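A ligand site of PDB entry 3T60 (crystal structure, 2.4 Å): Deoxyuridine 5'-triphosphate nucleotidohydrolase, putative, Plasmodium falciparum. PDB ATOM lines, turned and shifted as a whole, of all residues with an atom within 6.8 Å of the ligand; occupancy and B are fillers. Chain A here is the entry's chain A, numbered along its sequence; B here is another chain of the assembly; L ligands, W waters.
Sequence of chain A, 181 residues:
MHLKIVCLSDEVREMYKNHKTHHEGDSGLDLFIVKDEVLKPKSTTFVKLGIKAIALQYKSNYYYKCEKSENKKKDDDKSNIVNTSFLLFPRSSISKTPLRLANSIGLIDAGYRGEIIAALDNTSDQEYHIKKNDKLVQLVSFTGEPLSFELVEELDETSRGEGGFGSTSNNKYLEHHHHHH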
ATOM      1  N   PHE A  46      -8.377  21.106 -13.107  1.00  0.00           N
ATOM      2  CA  PHE A  46      -8.138  20.591 -14.436  1.00  0.00           C
ATOM      3  C   PHE A  46      -9.016  21.390 -15.411  1.00  0.00           C
ATOM      4  O   PHE A  46     -10.229  21.158 -15.525  1.00  0.00           O
ATOM      5  CB  PHE A  46      -8.330  19.054 -14.503  1.00  0.00           C
ATOM      6  CG  PHE A  46      -7.356  18.322 -13.586  1.00  0.00           C
ATOM      7  CD1 PHE A  46      -7.680  18.069 -12.262  1.00  0.00           C
ATOM      8  CD2 PHE A  46      -6.072  17.996 -14.026  1.00  0.00           C
ATOM      9  CE1 PHE A  46      -6.769  17.469 -11.406  1.00  0.00           C
ATOM     10  CE2 PHE A  46      -5.153  17.390 -13.187  1.00  0.00           C
ATOM     11  CZ  PHE A  46      -5.490  17.123 -11.865  1.00  0.00           C
ATOM     12  N   LYS A  48     -10.437  22.486 -18.753  1.00  0.00           N
ATOM     13  CA  LYS A  48     -10.609  22.000 -20.120  1.00  0.00           C
ATOM     14  C   LYS A  48     -10.638  23.123 -21.122  1.00  0.00           C
ATOM     15  O   LYS A  48     -11.348  24.146 -20.956  1.00  0.00           O
ATOM     16  CB  LYS A  48     -11.888  21.199 -20.216  1.00  0.00           C
ATOM     17  CG  LYS A  48     -11.842  19.884 -19.500  1.00  0.00           C
ATOM     18  CD  LYS A  48     -13.286  19.322 -19.370  1.00  0.00           C
ATOM     19  CE  LYS A  48     -13.464  18.371 -18.153  1.00  0.00           C
ATOM     20  NZ  LYS A  48     -14.951  18.072 -17.923  1.00  0.00           N
ATOM     21  N   LEU A  88       2.861  21.157 -23.909  1.00  0.00           N
ATOM     22  CA  LEU A  88       2.050  22.186 -23.401  1.00  0.00           C
ATOM     23  C   LEU A  88       2.824  23.024 -22.390  1.00  0.00           C
ATOM     24  O   LEU A  88       3.105  22.560 -21.282  1.00  0.00           O
ATOM     25  CB  LEU A  88       0.775  21.617 -22.836  1.00  0.00           C
ATOM     26  CG  LEU A  88      -0.210  22.697 -22.310  1.00  0.00           C
ATOM     27  CD1 LEU A  88      -1.154  23.093 -23.425  1.00  0.00           C
ATOM     28  CD2 LEU A  88      -1.078  22.295 -21.165  1.00  0.00           C
ATOM     29  N   LEU A 101       1.588  25.762 -13.533  1.00  0.00           N
ATOM     30  CA  LEU A 101       1.304  24.493 -14.212  1.00  0.00           C
ATOM     31  C   LEU A 101       1.744  23.286 -13.304  1.00  0.00           C
ATOM     32  O   LEU A 101       2.959  23.019 -13.129  1.00  0.00           O
ATOM     33  CB  LEU A 101       1.912  24.479 -15.639  1.00  0.00           C
ATOM     34  CG  LEU A 101       1.116  23.662 -16.655  1.00  0.00           C
ATOM     35  CD1 LEU A 101      -0.228  24.302 -17.035  1.00  0.00           C
ATOM     36  CD2 LEU A 101       1.948  23.285 -17.883  1.00  0.00           C
ATOM     37  N   ALA A 102       0.761  22.570 -12.741  1.00  0.00           N
ATOM     38  CA  ALA A 102       1.070  21.431 -11.847  1.00  0.00           C
ATOM     39  C   ALA A 102       2.174  20.510 -12.323  1.00  0.00           C
ATOM     40  O   ALA A 102       3.157  20.192 -11.527  1.00  0.00           O
ATOM     41  CB  ALA A 102      -0.212  20.636 -11.417  1.00  0.00           C
ATOM     42  N   ASN A 103       2.056  20.088 -13.594  1.00  0.00           N
ATOM     43  CA  ASN A 103       3.011  19.111 -14.179  1.00  0.00           C
ATOM     44  C   ASN A 103       4.190  19.730 -14.908  1.00  0.00           C
ATOM     45  O   ASN A 103       4.839  19.041 -15.682  1.00  0.00           O
ATOM     46  CB  ASN A 103       2.282  18.054 -15.051  1.00  0.00           C
ATOM     47  CG  ASN A 103       1.331  18.696 -16.112  1.00  0.00           C
ATOM     48  OD1 ASN A 103       0.676  19.760 -15.901  1.00  0.00           O
ATOM     49  ND2 ASN A 103       1.252  18.035 -17.264  1.00  0.00           N
ATOM     50  N   ILE A 105       5.534  21.050 -17.524  1.00  0.00           N
ATOM     51  CA  ILE A 105       5.329  21.041 -18.982  1.00  0.00           C
ATOM     52  C   ILE A 105       4.561  19.754 -19.235  1.00  0.00           C
ATOM     53  O   ILE A 105       4.967  18.704 -18.762  1.00  0.00           O
ATOM     54  CB  ILE A 105       6.618  20.983 -19.829  1.00  0.00           C
ATOM     55  CG1 ILE A 105       7.617  22.125 -19.457  1.00  0.00           C
ATOM     56  CG2 ILE A 105       6.295  20.973 -21.283  1.00  0.00           C
ATOM     57  CD1 ILE A 105       7.217  23.552 -19.787  1.00  0.00           C
ATOM     58  N   GLY A 106       3.452  19.855 -19.961  1.00  0.00           N
ATOM     59  CA  GLY A 106       2.637  18.742 -20.281  1.00  0.00           C
ATOM     60  C   GLY A 106       3.119  18.118 -21.543  1.00  0.00           C
ATOM     61  O   GLY A 106       3.435  18.798 -22.539  1.00  0.00           O
ATOM     62  N   LEU A 107       3.226  16.798 -21.487  1.00  0.00           N
ATOM     63  CA  LEU A 107       3.641  16.046 -22.622  1.00  0.00           C
ATOM     64  C   LEU A 107       2.413  15.409 -23.334  1.00  0.00           C
ATOM     65  O   LEU A 107       1.763  14.537 -22.796  1.00  0.00           O
ATOM     66  CB  LEU A 107       4.644  15.018 -22.158  1.00  0.00           C
ATOM     67  CG  LEU A 107       5.242  14.044 -23.171  1.00  0.00           C
ATOM     68  CD1 LEU A 107       6.121  14.768 -24.084  1.00  0.00           C
ATOM     69  CD2 LEU A 107       6.050  13.076 -22.322  1.00  0.00           C
ATOM     70  N   ILE A 108       2.082  15.860 -24.541  1.00  0.00           N
ATOM     71  CA  ILE A 108       0.918  15.269 -25.215  1.00  0.00           C
ATOM     72  C   ILE A 108       1.472  14.253 -26.223  1.00  0.00           C
ATOM     73  O   ILE A 108       2.251  14.643 -27.107  1.00  0.00           O
ATOM     74  CB  ILE A 108      -0.067  16.352 -25.712  1.00  0.00           C
ATOM     75  CG1 ILE A 108      -0.533  17.182 -24.476  1.00  0.00           C
ATOM     76  CG2 ILE A 108      -1.336  15.725 -26.423  1.00  0.00           C
ATOM     77  CD1 ILE A 108      -0.825  18.612 -24.734  1.00  0.00           C
ATOM     78  N   ASP A 109       1.261  12.961 -25.955  1.00  0.00           N
ATOM     79  CA  ASP A 109       1.669  11.849 -26.838  1.00  0.00           C
ATOM     80  C   ASP A 109       0.988  11.862 -28.200  1.00  0.00           C
ATOM     81  O   ASP A 109      -0.178  12.324 -28.313  1.00  0.00           O
ATOM     82  CB  ASP A 109       1.444  10.463 -26.178  1.00  0.00           C
ATOM     83  N   TYR A 112      -2.757  10.749 -28.730  1.00  0.00           N
ATOM     84  CA  TYR A 112      -3.762  11.232 -27.788  1.00  0.00           C
ATOM     85  C   TYR A 112      -4.872  12.002 -28.504  1.00  0.00           C
ATOM     86  O   TYR A 112      -4.578  12.910 -29.264  1.00  0.00           O
ATOM     87  CB  TYR A 112      -3.114  12.084 -26.702  1.00  0.00           C
ATOM     88  CG  TYR A 112      -4.066  12.577 -25.670  1.00  0.00           C
ATOM     89  CD1 TYR A 112      -4.606  11.722 -24.673  1.00  0.00           C
ATOM     90  CD2 TYR A 112      -4.498  13.896 -25.704  1.00  0.00           C
ATOM     91  CE1 TYR A 112      -5.549  12.213 -23.694  1.00  0.00           C
ATOM     92  CE2 TYR A 112      -5.398  14.378 -24.771  1.00  0.00           C
ATOM     93  CZ  TYR A 112      -5.926  13.538 -23.751  1.00  0.00           C
ATOM     94  OH  TYR A 112      -6.866  14.127 -22.837  1.00  0.00           O
ATOM     95  N   GLY A 114      -7.949  12.824 -26.639  1.00  0.00           N
ATOM     96  CA  GLY A 114      -8.781  13.486 -25.665  1.00  0.00           C
ATOM     97  C   GLY A 114      -8.714  15.020 -25.793  1.00  0.00           C
ATOM     98  O   GLY A 114      -7.879  15.617 -26.524  1.00  0.00           O
ATOM     99  N   GLU A 115      -9.640  15.644 -25.079  1.00  0.00           N
ATOM    100  CA  GLU A 115      -9.620  17.070 -24.894  1.00  0.00           C
ATOM    101  C   GLU A 115      -8.328  17.512 -24.181  1.00  0.00           C
ATOM    102  O   GLU A 115      -7.886  16.883 -23.198  1.00  0.00           O
ATOM    103  CB  GLU A 115     -10.825  17.545 -24.076  1.00  0.00           C
ATOM    104  CG  GLU A 115     -10.915  19.069 -23.997  1.00  0.00           C
ATOM    105  CD  GLU A 115     -12.206  19.515 -23.312  1.00  0.00           C
ATOM    106  OE1 GLU A 115     -12.683  20.668 -23.461  1.00  0.00           O
ATOM    107  OE2 GLU A 115     -12.755  18.670 -22.622  1.00  0.00           O
ATOM    108  N   ILE A 116      -7.769  18.598 -24.659  1.00  0.00           N
ATOM    109  CA  ILE A 116      -6.630  19.201 -24.000  1.00  0.00           C
ATOM    110  C   ILE A 116      -7.004  19.982 -22.717  1.00  0.00           C
ATOM    111  O   ILE A 116      -7.983  20.717 -22.638  1.00  0.00           O
ATOM    112  CB  ILE A 116      -5.803  19.959 -25.052  1.00  0.00           C
ATOM    113  CG1 ILE A 116      -5.342  18.922 -26.073  1.00  0.00           C
ATOM    114  CG2 ILE A 116      -4.627  20.697 -24.454  1.00  0.00           C
ATOM    115  CD1 ILE A 116      -4.966  19.539 -27.285  1.00  0.00           C
ATOM    116  N   ILE A 117      -6.238  19.704 -21.677  1.00  0.00           N
ATOM    117  CA  ILE A 117      -6.499  20.153 -20.302  1.00  0.00           C
ATOM    118  C   ILE A 117      -5.246  20.811 -19.758  1.00  0.00           C
ATOM    119  O   ILE A 117      -4.154  20.297 -19.949  1.00  0.00           O
ATOM    120  CB  ILE A 117      -6.882  18.929 -19.400  1.00  0.00           C
ATOM    121  CG1 ILE A 117      -8.246  18.380 -19.869  1.00  0.00           C
ATOM    122  CG2 ILE A 117      -7.063  19.307 -17.907  1.00  0.00           C
ATOM    123  CD1 ILE A 117      -8.719  17.210 -19.072  1.00  0.00           C
ATOM    124  N   ALA A 118      -5.415  21.941 -19.093  1.00  0.00           N
ATOM    125  CA  ALA A 118      -4.361  22.625 -18.327  1.00  0.00           C
ATOM    126  C   ALA A 118      -4.597  22.385 -16.852  1.00  0.00           C
ATOM    127  O   ALA A 118      -5.636  22.843 -16.309  1.00  0.00           O
ATOM    128  CB  ALA A 118      -4.407  24.101 -18.590  1.00  0.00           C
ATOM    129  N   ALA A 119      -3.660  21.714 -16.202  1.00  0.00           N
ATOM    130  CA  ALA A 119      -3.733  21.515 -14.736  1.00  0.00           C
ATOM    131  C   ALA A 119      -3.158  22.697 -13.962  1.00  0.00           C
ATOM    132  O   ALA A 119      -1.946  22.726 -13.714  1.00  0.00           O
ATOM    133  CB  ALA A 119      -2.961  20.212 -14.310  1.00  0.00           C
ATOM    134  N   ARG B  91       5.046  13.194 -14.440  1.00  0.00           N
ATOM    135  CA  ARG B  91       3.966  12.540 -15.135  1.00  0.00           C
ATOM    136  C   ARG B  91       2.721  13.412 -14.914  1.00  0.00           C
ATOM    137  O   ARG B  91       2.604  14.117 -13.889  1.00  0.00           O
ATOM    138  CB  ARG B  91       3.791  11.094 -14.615  1.00  0.00           C
ATOM    139  CG  ARG B  91       4.670  10.074 -15.301  1.00  0.00           C
ATOM    140  CD  ARG B  91       4.440   8.622 -14.759  1.00  0.00           C
ATOM    141  NE  ARG B  91       3.340   7.898 -15.395  1.00  0.00           N
ATOM    142  CZ  ARG B  91       2.186   7.638 -14.795  1.00  0.00           C
ATOM    143  NH1 ARG B  91       1.967   8.019 -13.539  1.00  0.00           N
ATOM    144  NH2 ARG B  91       1.208   7.024 -15.468  1.00  0.00           N
ATOM    145  N   SER B  92       1.809  13.420 -15.864  1.00  0.00           N
ATOM    146  CA  SER B  92       0.591  14.182 -15.755  1.00  0.00           C
ATOM    147  C   SER B  92      -0.076  13.944 -14.410  1.00  0.00           C
ATOM    148  O   SER B  92      -0.808  14.785 -13.850  1.00  0.00           O
ATOM    149  CB  SER B  92      -0.390  13.708 -16.842  1.00  0.00           C
ATOM    150  OG  SER B  92       0.134  14.015 -18.103  1.00  0.00           O
ATOM    151  N   SER B  93       0.095  12.728 -13.933  1.00  0.00           N
ATOM    152  CA  SER B  93      -0.692  12.280 -12.804  1.00  0.00           C
ATOM    153  C   SER B  93      -0.166  12.810 -11.461  1.00  0.00           C
ATOM    154  O   SER B  93      -0.934  12.737 -10.436  1.00  0.00           O
ATOM    155  CB  SER B  93      -0.794  10.734 -12.792  1.00  0.00           C
ATOM    156  OG  SER B  93       0.451  10.187 -12.558  1.00  0.00           O
ATOM    157  N   ILE B  94       1.059  13.413 -11.487  1.00  0.00           N
ATOM    158  CA  ILE B  94       1.660  14.140 -10.358  1.00  0.00           C
ATOM    159  C   ILE B  94       0.700  15.233  -9.929  1.00  0.00           C
ATOM    160  O   ILE B  94       0.602  15.575  -8.731  1.00  0.00           O
ATOM    161  CB  ILE B  94       3.105  14.745 -10.661  1.00  0.00           C
ATOM    162  CG1 ILE B  94       3.982  14.752  -9.400  1.00  0.00           C
ATOM    163  CG2 ILE B  94       3.022  16.159 -11.347  1.00  0.00           C
ATOM    164  CD1 ILE B  94       5.501  15.004  -9.588  1.00  0.00           C
ATOM    165  N   SER B  95      -0.077  15.733 -10.897  1.00  0.00           N
ATOM    166  CA  SER B  95      -0.922  16.890 -10.677  1.00  0.00           C
ATOM    167  C   SER B  95      -2.063  16.556  -9.737  1.00  0.00           C
ATOM    168  O   SER B  95      -2.704  17.423  -9.178  1.00  0.00           O
ATOM    169  CB  SER B  95      -1.456  17.404 -11.998  1.00  0.00           C
ATOM    170  OG  SER B  95      -2.454  16.487 -12.454  1.00  0.00           O
ATOM    171  N   LYS B  96      -2.293  15.263  -9.568  1.00  0.00           N
ATOM    172  CA  LYS B  96      -3.323  14.803  -8.662  1.00  0.00           C
ATOM    173  C   LYS B  96      -2.740  14.643  -7.240  1.00  0.00           C
ATOM    174  O   LYS B  96      -3.490  14.346  -6.316  1.00  0.00           O
ATOM    175  CB  LYS B  96      -3.978  13.494  -9.188  1.00  0.00           C
HETATM  176  N1  LIG L   1      -2.404  16.108 -21.206  1.00  0.00           N
HETATM  177  O1  LIG L   1      -2.428  11.530 -21.531  1.00  0.00           O
HETATM  178  C1  LIG L   1      -3.026  17.352 -21.199  1.00  0.00           C
HETATM  179  N2  LIG L   1      -5.223  13.518 -18.334  1.00  0.00           N
HETATM  180  O2  LIG L   1      -4.111  17.453 -21.730  1.00  0.00           O
HETATM  181  N3  LIG L   1      -2.414  18.413 -20.646  1.00  0.00           N
HETATM  182  C2  LIG L   1      -1.216  18.273 -20.083  1.00  0.00           C
HETATM  183  O3  LIG L   1      -0.682  19.242 -19.547  1.00  0.00           O
HETATM  184  C3  LIG L   1      -0.562  17.021 -20.038  1.00  0.00           C
HETATM  185  C4  LIG L   1      -1.199  15.918 -20.613  1.00  0.00           C
HETATM  186  C5  LIG L   1      -3.070  14.928 -21.699  1.00  0.00           C
HETATM  187  C6  LIG L   1      -5.093  14.004 -16.976  1.00  0.00           C
HETATM  188  C7  LIG L   1      -6.618  14.269 -16.718  1.00  0.00           C
HETATM  189  C8  LIG L   1      -7.622  13.485 -17.347  1.00  0.00           C
HETATM  190  C9  LIG L   1      -2.413  13.848 -22.468  1.00  0.00           C
HETATM  191  C10 LIG L   1      -9.010  13.680 -17.107  1.00  0.00           C
HETATM  192  C11 LIG L   1      -9.482  14.675 -16.249  1.00  0.00           C
HETATM  193  C12 LIG L   1      -8.511  15.463 -15.614  1.00  0.00           C
HETATM  194  C13 LIG L   1      -7.136  15.237 -15.838  1.00  0.00           C
HETATM  195  C14 LIG L   1      -4.298  15.230 -16.794  1.00  0.00           C
HETATM  196  C15 LIG L   1      -3.160  15.422 -15.978  1.00  0.00           C
HETATM  197  C16 LIG L   1      -2.432  16.609 -16.009  1.00  0.00           C
HETATM  198  C17 LIG L   1      -2.835  17.638 -16.841  1.00  0.00           C
HETATM  199  C18 LIG L   1      -3.942  17.472 -17.663  1.00  0.00           C
HETATM  200  C19 LIG L   1      -4.664  16.283 -17.663  1.00  0.00           C
HETATM  201  C20 LIG L   1      -2.588  12.907 -21.241  1.00  0.00           C
HETATM  202  C21 LIG L   1      -4.805  12.961 -15.893  1.00  0.00           C
HETATM  203  C22 LIG L   1      -3.928  11.918 -16.193  1.00  0.00           C
HETATM  204  C23 LIG L   1      -3.612  10.907 -15.269  1.00  0.00           C
HETATM  205  C24 LIG L   1      -4.162  10.922 -13.976  1.00  0.00           C
HETATM  206  C25 LIG L   1      -5.015  11.948 -13.603  1.00  0.00           C
HETATM  207  C26 LIG L   1      -5.285  12.961 -14.563  1.00  0.00           C
HETATM  208  C27 LIG L   1      -3.952  13.163 -20.585  1.00  0.00           C
HETATM  209  O4  LIG L   1      -4.248  14.477 -21.025  1.00  0.00           O
HETATM  210  C28 LIG L   1      -3.980  13.092 -19.036  1.00  0.00           C
HETATM  211  O   HOH W   1      -1.388  20.926 -17.495  1.00  0.00           O
HETATM  212  O   HOH W   2       2.237  15.404 -19.107  1.00  0.00           O
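OH of Tyr 112 lies within hydrogen-bond range of O of Glu 115 (3.0 Å). The side-chain hydroxyl (OG) of Ser 95 of chain B sits at hydrogen-bond distance from the backbone carbonyl oxygen (O) of Ser 92 of chain B, 2.7 Å away. O of Gly 106 lies within hydrogen-bond range of N of Leu 88 (2.8 Å). OG of Ser 93 of chain B lies within hydrogen-bond range of NH1 of Arg 91 of chain B. The backbone carbonyl oxygen of Ala 119 sits at hydrogen-bond distance from the backbone NH of Ala 102 (2.9 Å).
The backbone NH of Ile 117 lies within hydrogen-bond range of an oxygen (O2) of the ligand (3.1 Å). A nitrogen (N3) of the ligand is in hydrogen-bond range of the backbone carbonyl oxygen (O) of Ile 117, at 2.7 Å. O4 of the ligand lies within hydrogen-bond range of OH of Tyr 112. The side-chain amide nitrogen of Asn 103 is in hydrogen-bond range of an oxygen (O3) of the ligand (3.2 Å).
CD2 of Phe 46 touches C13 of the ligand, at 3.5 Å. Leu 88 touches the ligand. CA of Gly 106 touches O3 of the ligand (3.4 Å). Leu 107 touches the ligand. CG1 of Ile 108 touches N1 of the ligand, 3.9 Å away. Ile 116 touches the ligand (CA to O2, 3.8 Å). CB of Ala 119 touches C17 of the ligand, 3.6 Å away. O of Ser 92 of chain B touches C15 of the ligand, at 3.2 Å. Ser 93 of chain B touches the ligand (CB to C24, 3.6 Å). OG of Ser 95 of chain B touches C16 of the ligand (3.6 Å). Hydrophobic or aromatic side chains that line the ligand: Phe 46, Leu 88, Ile 108, Tyr 112, Ile 117 and Ala 119. The nearest printed residue that does not touch the ligand is Glu 115 (4.1 Å).
Water W1 lies within hydrogen-bond range of N of Ala 119 (2.7 Å), O3 of the ligand (2.7 Å) and OD1 of Asn 103 (2.9 Å). Water W2 lies within hydrogen-bond range of OG of Ser 92 of chain B (2.7 Å), N of Leu 107 (2.9 Å) and ND2 of Asn 103 (3.4 Å).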
